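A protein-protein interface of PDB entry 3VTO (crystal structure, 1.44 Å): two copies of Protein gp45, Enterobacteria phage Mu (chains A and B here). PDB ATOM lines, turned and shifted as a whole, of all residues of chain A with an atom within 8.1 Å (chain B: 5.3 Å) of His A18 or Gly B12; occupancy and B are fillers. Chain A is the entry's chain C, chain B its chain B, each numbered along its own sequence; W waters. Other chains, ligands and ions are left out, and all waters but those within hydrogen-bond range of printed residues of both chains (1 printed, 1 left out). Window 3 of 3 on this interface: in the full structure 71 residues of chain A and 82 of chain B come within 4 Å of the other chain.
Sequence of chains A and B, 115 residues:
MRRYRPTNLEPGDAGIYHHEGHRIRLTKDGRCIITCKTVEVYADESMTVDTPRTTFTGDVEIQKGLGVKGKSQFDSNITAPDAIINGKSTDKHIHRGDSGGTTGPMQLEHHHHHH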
ATOM      1  N   ARG A   5     -35.264 -23.717 -16.761  1.00  0.00           N
ATOM      2  CA  ARG A   5     -34.147 -24.597 -16.420  1.00  0.00           C
ATOM      3  C   ARG A   5     -34.527 -25.472 -15.243  1.00  0.00           C
ATOM      4  O   ARG A   5     -34.029 -25.274 -14.115  1.00  0.00           O
ATOM      5  CB  ARG A   5     -32.928 -23.772 -16.059  1.00  0.00           C
ATOM      6  CG  ARG A   5     -32.412 -22.938 -17.167  1.00  0.00           C
ATOM      7  CD  ARG A   5     -31.753 -23.797 -18.230  1.00  0.00           C
ATOM      8  NE  ARG A   5     -31.067 -22.803 -18.986  1.00  0.00           N
ATOM      9  CZ  ARG A   5     -31.728 -22.038 -19.830  1.00  0.00           C
ATOM     10  NH1 ARG A   5     -31.131 -21.056 -20.439  1.00  0.00           N
ATOM     11  NH2 ARG A   5     -33.000 -22.317 -20.051  1.00  0.00           N
ATOM     12  N   PRO A   6     -35.399 -26.439 -15.513  1.00  0.00           N
ATOM     13  CA  PRO A   6     -35.838 -27.298 -14.424  1.00  0.00           C
ATOM     14  C   PRO A   6     -34.676 -28.078 -13.805  1.00  0.00           C
ATOM     15  O   PRO A   6     -33.667 -28.385 -14.502  1.00  0.00           O
ATOM     16  CB  PRO A   6     -36.876 -28.210 -15.082  1.00  0.00           C
ATOM     17  CG  PRO A   6     -36.414 -28.257 -16.561  1.00  0.00           C
ATOM     18  CD  PRO A   6     -35.968 -26.825 -16.824  1.00  0.00           C
ATOM     19  N   THR A   7     -34.808 -28.343 -12.495  1.00  0.00           N
ATOM     20  CA  THR A   7     -33.728 -28.962 -11.714  1.00  0.00           C
ATOM     21  C   THR A   7     -34.189 -30.238 -11.009  1.00  0.00           C
ATOM     22  O   THR A   7     -33.382 -30.893 -10.350  1.00  0.00           O
ATOM     23  CB  THR A   7     -33.166 -28.008 -10.615  1.00  0.00           C
ATOM     24  OG1 THR A   7     -34.143 -27.841  -9.577  1.00  0.00           O
ATOM     25  CG2 THR A   7     -32.764 -26.668 -11.166  1.00  0.00           C
ATOM     26  N   GLY A  15     -28.726 -38.575 -17.585  1.00  0.00           N
ATOM     27  CA  GLY A  15     -28.655 -37.285 -18.252  1.00  0.00           C
ATOM     28  C   GLY A  15     -27.272 -36.736 -18.445  1.00  0.00           C
ATOM     29  O   GLY A  15     -26.254 -37.372 -18.075  1.00  0.00           O
ATOM     30  N   ILE A  16     -27.278 -35.564 -19.052  1.00  0.00           N
ATOM     31  CA  ILE A  16     -26.090 -34.734 -19.276  1.00  0.00           C
ATOM     32  C   ILE A  16     -26.478 -33.390 -18.671  1.00  0.00           C
ATOM     33  O   ILE A  16     -27.502 -32.826 -19.036  1.00  0.00           O
ATOM     34  CB  ILE A  16     -25.781 -34.566 -20.765  1.00  0.00           C
ATOM     35  CG1 ILE A  16     -25.555 -35.900 -21.444  1.00  0.00           C
ATOM     36  CG2 ILE A  16     -24.579 -33.665 -20.964  1.00  0.00           C
ATOM     37  CD1 ILE A  16     -25.589 -35.837 -22.970  1.00  0.00           C
ATOM     38  N   TYR A  17     -25.679 -32.918 -17.712  1.00  0.00           N
ATOM     39  CA  TYR A  17     -26.065 -31.800 -16.871  1.00  0.00           C
ATOM     40  C   TYR A  17     -24.988 -30.745 -16.848  1.00  0.00           C
ATOM     41  O   TYR A  17     -23.871 -31.052 -16.501  1.00  0.00           O
ATOM     42  CB  TYR A  17     -26.240 -32.268 -15.438  1.00  0.00           C
ATOM     43  CG  TYR A  17     -27.187 -33.397 -15.323  1.00  0.00           C
ATOM     44  CD1 TYR A  17     -28.558 -33.160 -15.271  1.00  0.00           C
ATOM     45  CD2 TYR A  17     -26.726 -34.706 -15.281  1.00  0.00           C
ATOM     46  CE1 TYR A  17     -29.485 -34.227 -15.122  1.00  0.00           C
ATOM     47  CE2 TYR A  17     -27.628 -35.778 -15.137  1.00  0.00           C
ATOM     48  CZ  TYR A  17     -29.006 -35.523 -15.091  1.00  0.00           C
ATOM     49  OH  TYR A  17     -29.975 -36.503 -14.943  1.00  0.00           O
ATOM     50  N   HIS A  18     -25.359 -29.505 -17.133  1.00  0.00           N
ATOM     51  CA  HIS A  18     -24.415 -28.405 -16.979  1.00  0.00           C
ATOM     52  C   HIS A  18     -24.716 -27.652 -15.675  1.00  0.00           C
ATOM     53  O   HIS A  18     -25.891 -27.484 -15.311  1.00  0.00           O
ATOM     54  CB  HIS A  18     -24.538 -27.458 -18.169  1.00  0.00           C
ATOM     55  CG  HIS A  18     -23.402 -26.490 -18.276  1.00  0.00           C
ATOM     56  ND1 HIS A  18     -23.300 -25.354 -17.490  1.00  0.00           N
ATOM     57  CD2 HIS A  18     -22.296 -26.511 -19.061  1.00  0.00           C
ATOM     58  CE1 HIS A  18     -22.178 -24.710 -17.810  1.00  0.00           C
ATOM     59  NE2 HIS A  18     -21.558 -25.394 -18.759  1.00  0.00           N
ATOM     60  N   HIS A  19     -23.670 -27.185 -14.995  1.00  0.00           N
ATOM     61  CA  HIS A  19     -23.850 -26.510 -13.708  1.00  0.00           C
ATOM     62  C   HIS A  19     -24.701 -25.241 -13.755  1.00  0.00           C
ATOM     63  O   HIS A  19     -25.296 -24.833 -12.728  1.00  0.00           O
ATOM     64  CB  HIS A  19     -22.498 -26.225 -13.039  1.00  0.00           C
ATOM     65  CG  HIS A  19     -21.737 -25.101 -13.665  1.00  0.00           C
ATOM     66  ND1 HIS A  19     -21.975 -23.780 -13.353  1.00  0.00           N
ATOM     67  CD2 HIS A  19     -20.734 -25.100 -14.574  1.00  0.00           C
ATOM     68  CE1 HIS A  19     -21.153 -23.014 -14.049  1.00  0.00           C
ATOM     69  NE2 HIS A  19     -20.392 -23.792 -14.801  1.00  0.00           N
ATOM     70  N   GLU A  20     -24.770 -24.608 -14.929  1.00  0.00           N
ATOM     71  CA  GLU A  20     -25.637 -23.443 -15.094  1.00  0.00           C
ATOM     72  C   GLU A  20     -27.115 -23.783 -15.030  1.00  0.00           C
ATOM     73  O   GLU A  20     -27.948 -22.909 -14.776  1.00  0.00           O
ATOM     74  CB  GLU A  20     -25.388 -22.682 -16.387  1.00  0.00           C
ATOM     75  CG  GLU A  20     -24.094 -22.010 -16.438  1.00  0.00           C
ATOM     76  CD  GLU A  20     -23.801 -21.453 -17.834  1.00  0.00           C
ATOM     77  OE1 GLU A  20     -24.688 -21.490 -18.719  1.00  0.00           O
ATOM     78  OE2 GLU A  20     -22.658 -21.009 -18.062  1.00  0.00           O
ATOM     79  N   GLY A  21     -27.429 -25.041 -15.312  1.00  0.00           N
ATOM     80  CA  GLY A  21     -28.793 -25.547 -15.084  1.00  0.00           C
ATOM     81  C   GLY A  21     -29.418 -26.215 -16.304  1.00  0.00           C
ATOM     82  O   GLY A  21     -30.373 -26.967 -16.176  1.00  0.00           O
ATOM     83  N   HIS A  22     -28.910 -25.938 -17.491  1.00  0.00           N
ATOM     84  CA  HIS A  22     -29.398 -26.602 -18.722  1.00  0.00           C
ATOM     85  C   HIS A  22     -28.972 -28.062 -18.738  1.00  0.00           C
ATOM     86  O   HIS A  22     -27.945 -28.410 -18.140  1.00  0.00           O
ATOM     87  CB  HIS A  22     -29.003 -25.872 -20.009  1.00  0.00           C
ATOM     88  CG  HIS A  22     -27.553 -25.549 -20.174  1.00  0.00           C
ATOM     89  ND1 HIS A  22     -26.840 -24.785 -19.269  1.00  0.00           N
ATOM     90  CD2 HIS A  22     -26.695 -25.866 -21.175  1.00  0.00           C
ATOM     91  CE1 HIS A  22     -25.624 -24.562 -19.759  1.00  0.00           C
ATOM     92  NE2 HIS A  22     -25.504 -25.228 -20.905  1.00  0.00           N
ATOM     93  N   ARG A  23     -29.799 -28.930 -19.347  1.00  0.00           N
ATOM     94  CA  ARG A  23     -29.540 -30.350 -19.273  1.00  0.00           C
ATOM     95  C   ARG A  23     -30.309 -31.117 -20.368  1.00  0.00           C
ATOM     96  O   ARG A  23     -31.257 -30.614 -20.994  1.00  0.00           O
ATOM     97  CB  ARG A  23     -29.989 -30.934 -17.917  1.00  0.00           C
ATOM     98  CG  ARG A  23     -31.492 -30.946 -17.730  1.00  0.00           C
ATOM     99  CD  ARG A  23     -31.857 -31.136 -16.257  1.00  0.00           C
ATOM    100  NE  ARG A  23     -33.298 -31.255 -16.089  1.00  0.00           N
ATOM    101  CZ  ARG A  23     -33.902 -31.545 -14.937  1.00  0.00           C
ATOM    102  NH1 ARG A  23     -33.165 -31.753 -13.859  1.00  0.00           N
ATOM    103  NH2 ARG A  23     -35.233 -31.612 -14.885  1.00  0.00           N
ATOM    104  N   ILE A  24     -29.854 -32.336 -20.576  1.00  0.00           N
ATOM    105  CA  ILE A  24     -30.550 -33.319 -21.389  1.00  0.00           C
ATOM    106  C   ILE A  24     -30.886 -34.453 -20.429  1.00  0.00           C
ATOM    107  O   ILE A  24     -29.985 -35.041 -19.789  1.00  0.00           O
ATOM    108  CB  ILE A  24     -29.653 -33.828 -22.547  1.00  0.00           C
ATOM    109  CG1 ILE A  24     -29.295 -32.676 -23.478  1.00  0.00           C
ATOM    110  CG2 ILE A  24     -30.329 -34.986 -23.295  1.00  0.00           C
ATOM    111  CD1 ILE A  24     -28.176 -33.018 -24.492  1.00  0.00           C
ATOM    112  N   THR A  35     -33.585 -29.063 -21.962  1.00  0.00           N
ATOM    113  CA  THR A  35     -33.964 -27.716 -21.513  1.00  0.00           C
ATOM    114  C   THR A  35     -32.714 -26.828 -21.561  1.00  0.00           C
ATOM    115  O   THR A  35     -31.724 -27.106 -20.873  1.00  0.00           O
ATOM    116  CB  THR A  35     -34.579 -27.772 -20.080  1.00  0.00           C
ATOM    117  OG1 THR A  35     -33.789 -28.672 -19.264  1.00  0.00           O
ATOM    118  CG2 THR A  35     -36.016 -28.273 -20.169  1.00  0.00           C
ATOM    119  N   GLU B  10     -14.334 -26.382 -22.848  1.00  0.00           N
ATOM    120  CA  GLU B  10     -14.230 -25.372 -21.808  1.00  0.00           C
ATOM    121  C   GLU B  10     -14.452 -25.997 -20.446  1.00  0.00           C
ATOM    122  O   GLU B  10     -15.157 -27.032 -20.330  1.00  0.00           O
ATOM    123  CB  GLU B  10     -15.297 -24.297 -21.994  1.00  0.00           C
ATOM    124  CG  GLU B  10     -15.195 -23.490 -23.268  1.00  0.00           C
ATOM    125  CD  GLU B  10     -14.077 -22.476 -23.188  1.00  0.00           C
ATOM    126  OE1 GLU B  10     -13.754 -22.067 -22.041  1.00  0.00           O
ATOM    127  OE2 GLU B  10     -13.539 -22.092 -24.252  1.00  0.00           O
ATOM    128  N   PRO B  11     -13.906 -25.353 -19.403  1.00  0.00           N
ATOM    129  CA  PRO B  11     -14.270 -25.671 -18.034  1.00  0.00           C
ATOM    130  C   PRO B  11     -15.786 -25.688 -17.862  1.00  0.00           C
ATOM    131  O   PRO B  11     -16.509 -24.775 -18.292  1.00  0.00           O
ATOM    132  CB  PRO B  11     -13.628 -24.539 -17.191  1.00  0.00           C
ATOM    133  CG  PRO B  11     -12.550 -23.946 -18.054  1.00  0.00           C
ATOM    134  CD  PRO B  11     -12.907 -24.261 -19.497  1.00  0.00           C
ATOM    135  N   GLY B  12     -16.259 -26.757 -17.258  1.00  0.00           N
ATOM    136  CA  GLY B  12     -17.681 -26.868 -16.959  1.00  0.00           C
ATOM    137  C   GLY B  12     -18.469 -27.587 -18.032  1.00  0.00           C
ATOM    138  O   GLY B  12     -19.615 -27.990 -17.776  1.00  0.00           O
ATOM    139  N   ASP B  13     -17.867 -27.857 -19.187  1.00  0.00           N
ATOM    140  CA  ASP B  13     -18.580 -28.624 -20.230  1.00  0.00           C
ATOM    141  C   ASP B  13     -19.027 -30.005 -19.719  1.00  0.00           C
ATOM    142  O   ASP B  13     -18.335 -30.660 -18.911  1.00  0.00           O
ATOM    143  CB  ASP B  13     -17.714 -28.808 -21.477  1.00  0.00           C
ATOM    144  CG  ASP B  13     -17.574 -27.536 -22.297  1.00  0.00           C
ATOM    145  OD1 ASP B  13     -18.155 -26.490 -21.949  1.00  0.00           O
ATOM    146  OD2 ASP B  13     -16.875 -27.616 -23.327  1.00  0.00           O
ATOM    147  N   ALA B  14     -20.164 -30.454 -20.225  1.00  0.00           N
ATOM    148  CA  ALA B  14     -20.731 -31.758 -19.893  1.00  0.00           C
ATOM    149  C   ALA B  14     -21.162 -32.348 -21.232  1.00  0.00           C
ATOM    150  O   ALA B  14     -21.809 -31.674 -22.004  1.00  0.00           O
ATOM    151  CB  ALA B  14     -21.903 -31.633 -18.966  1.00  0.00           C
ATOM    152  N   LEU B  26     -22.899 -29.806 -23.756  1.00  0.00           N
ATOM    153  CA  LEU B  26     -23.494 -28.649 -23.111  1.00  0.00           C
ATOM    154  C   LEU B  26     -22.385 -27.754 -22.616  1.00  0.00           C
ATOM    155  O   LEU B  26     -21.449 -28.217 -21.978  1.00  0.00           O
ATOM    156  CB  LEU B  26     -24.351 -29.064 -21.915  1.00  0.00           C
ATOM    157  CG  LEU B  26     -25.475 -30.049 -22.165  1.00  0.00           C
ATOM    158  CD1 LEU B  26     -26.298 -30.228 -20.913  1.00  0.00           C
ATOM    159  CD2 LEU B  26     -26.348 -29.632 -23.317  1.00  0.00           C
ATOM    160  N   THR B  27     -22.471 -26.481 -22.970  1.00  0.00           N
ATOM    161  CA  THR B  27     -21.380 -25.546 -22.658  1.00  0.00           C
ATOM    162  C   THR B  27     -21.957 -24.237 -22.109  1.00  0.00           C
ATOM    163  O   THR B  27     -23.152 -24.105 -21.926  1.00  0.00           O
ATOM    164  CB  THR B  27     -20.409 -25.365 -23.869  1.00  0.00           C
ATOM    165  OG1 THR B  27     -19.238 -24.645 -23.446  1.00  0.00           O
ATOM    166  CG2 THR B  27     -21.050 -24.654 -25.067  1.00  0.00           C
ATOM    167  N   LYS B  28     -21.104 -23.275 -21.816  1.00  0.00           N
ATOM    168  CA  LYS B  28     -21.531 -22.116 -21.063  1.00  0.00           C
ATOM    169  C   LYS B  28     -22.567 -21.301 -21.825  1.00  0.00           C
ATOM    170  O   LYS B  28     -22.706 -21.359 -23.071  1.00  0.00           O
ATOM    171  CB  LYS B  28     -20.330 -21.212 -20.670  1.00  0.00           C
ATOM    172  CG  LYS B  28     -19.568 -20.601 -21.733  1.00  0.00           C
ATOM    173  CD  LYS B  28     -18.431 -19.830 -21.086  1.00  0.00           C
ATOM    174  CE  LYS B  28     -17.450 -19.414 -22.138  1.00  0.00           C
ATOM    175  NZ  LYS B  28     -16.287 -18.631 -21.582  1.00  0.00           N
HETATM  176  O   HOH W   1     -19.017 -24.881 -19.875  1.00  0.00           O
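The backbone carbonyl oxygen (O) of Gly B12 lies close to a ring nitrogen (NE2) of His A18.
O of Thr B27 lies within hydrogen-bond range of NE2 of His A22, at 2.8 Å.
Of the 14 printed residues of chain A, 6 touch a printed residue of chain B.
Hydrophobic or aromatic side chains of chain A within 4 Å of the printed part of chain B: Ile A16, His A18 and His A22.
Of the 8 printed residues of chain B, 5 touch a printed residue of chain A.
Among the printed residues, 11 pairs touch across the chains.
Among the printed residues, no Asp or Glu carboxylate lies within 4 Å of a Lys or Arg side-chain nitrogen of the other chain.
OD1 of Asp B13 sits at hydrogen-bond distance from OG1 of Thr B27, at 2.6 Å.
The backbone carbonyl oxygen of Ala B14 sits at hydrogen-bond distance from the backbone NH of Leu B26, 2.8 Å away.
O of Pro A6 lies close to NE of Arg A23 (3.3 Å).
The backbone NH (N) of Ile A24 is in hydrogen-bond range of the backbone carbonyl oxygen (O) of Ile A16 (2.9 Å).
N of Glu A20 lies within hydrogen-bond range of ND1 of His A18, 3.0 Å away.
The backbone carbonyl oxygen (O) of Arg A23 sits at hydrogen-bond distance from the backbone NH (N) of Thr A35, at 3.0 Å.
Water W1 lies within hydrogen-bond range of OD1 of Asp B13 (2.8 Å), NE2 of His A18 (2.8 Å), O of Pro B11 (3.0 Å) and N of Lys B28 (3.3 Å).
Among the printed residues, merely in contact across the chains: Tyr A17 with Ala B14, Glu A20 with Lys B28, Ile A16 with Leu B26, His A18 with Leu B26, Ile A16 with Ala B14, His A18 with Thr B27, Arg A23 with Leu B26, His A22 with Leu B26 and His A18 with Lys B28.
No position is printed for both chains.
Of the 11 pairs that touch across the chains among the printed residues, none has its exchanged pair printed and touching as well.
Of the printed residues of chain B, Ile A16 touches Ala B14 (3.6 Å) and Leu B26 (3.4 Å).
Of the printed residues of chain B, Tyr A17 touches Ala B14.
Of chain B, only Gly B12 (3.3 Å), Leu B26 (3.5 Å), Thr B27 (3.6 Å) and Lys B28 (3.7 Å) come within 4 Å of His A18.
Printed residues of chain B within 4 Å of Glu A20: Lys B28.
Gly B12 touches one residue of chain A.
Of the printed residues of chain A, Lys B28 touches His A18 (3.7 Å) and Glu A20 (3.4 Å).
The nearest printed residue of chain B that does not touch His A18 is Asp B13 (4.4 Å).
The nearest printed residue of chain A that does not touch Gly B12 is His A19 (4.3 Å).
The nearest printed residue of chain B that does not touch His A22 is Lys B28 (4.9 Å).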
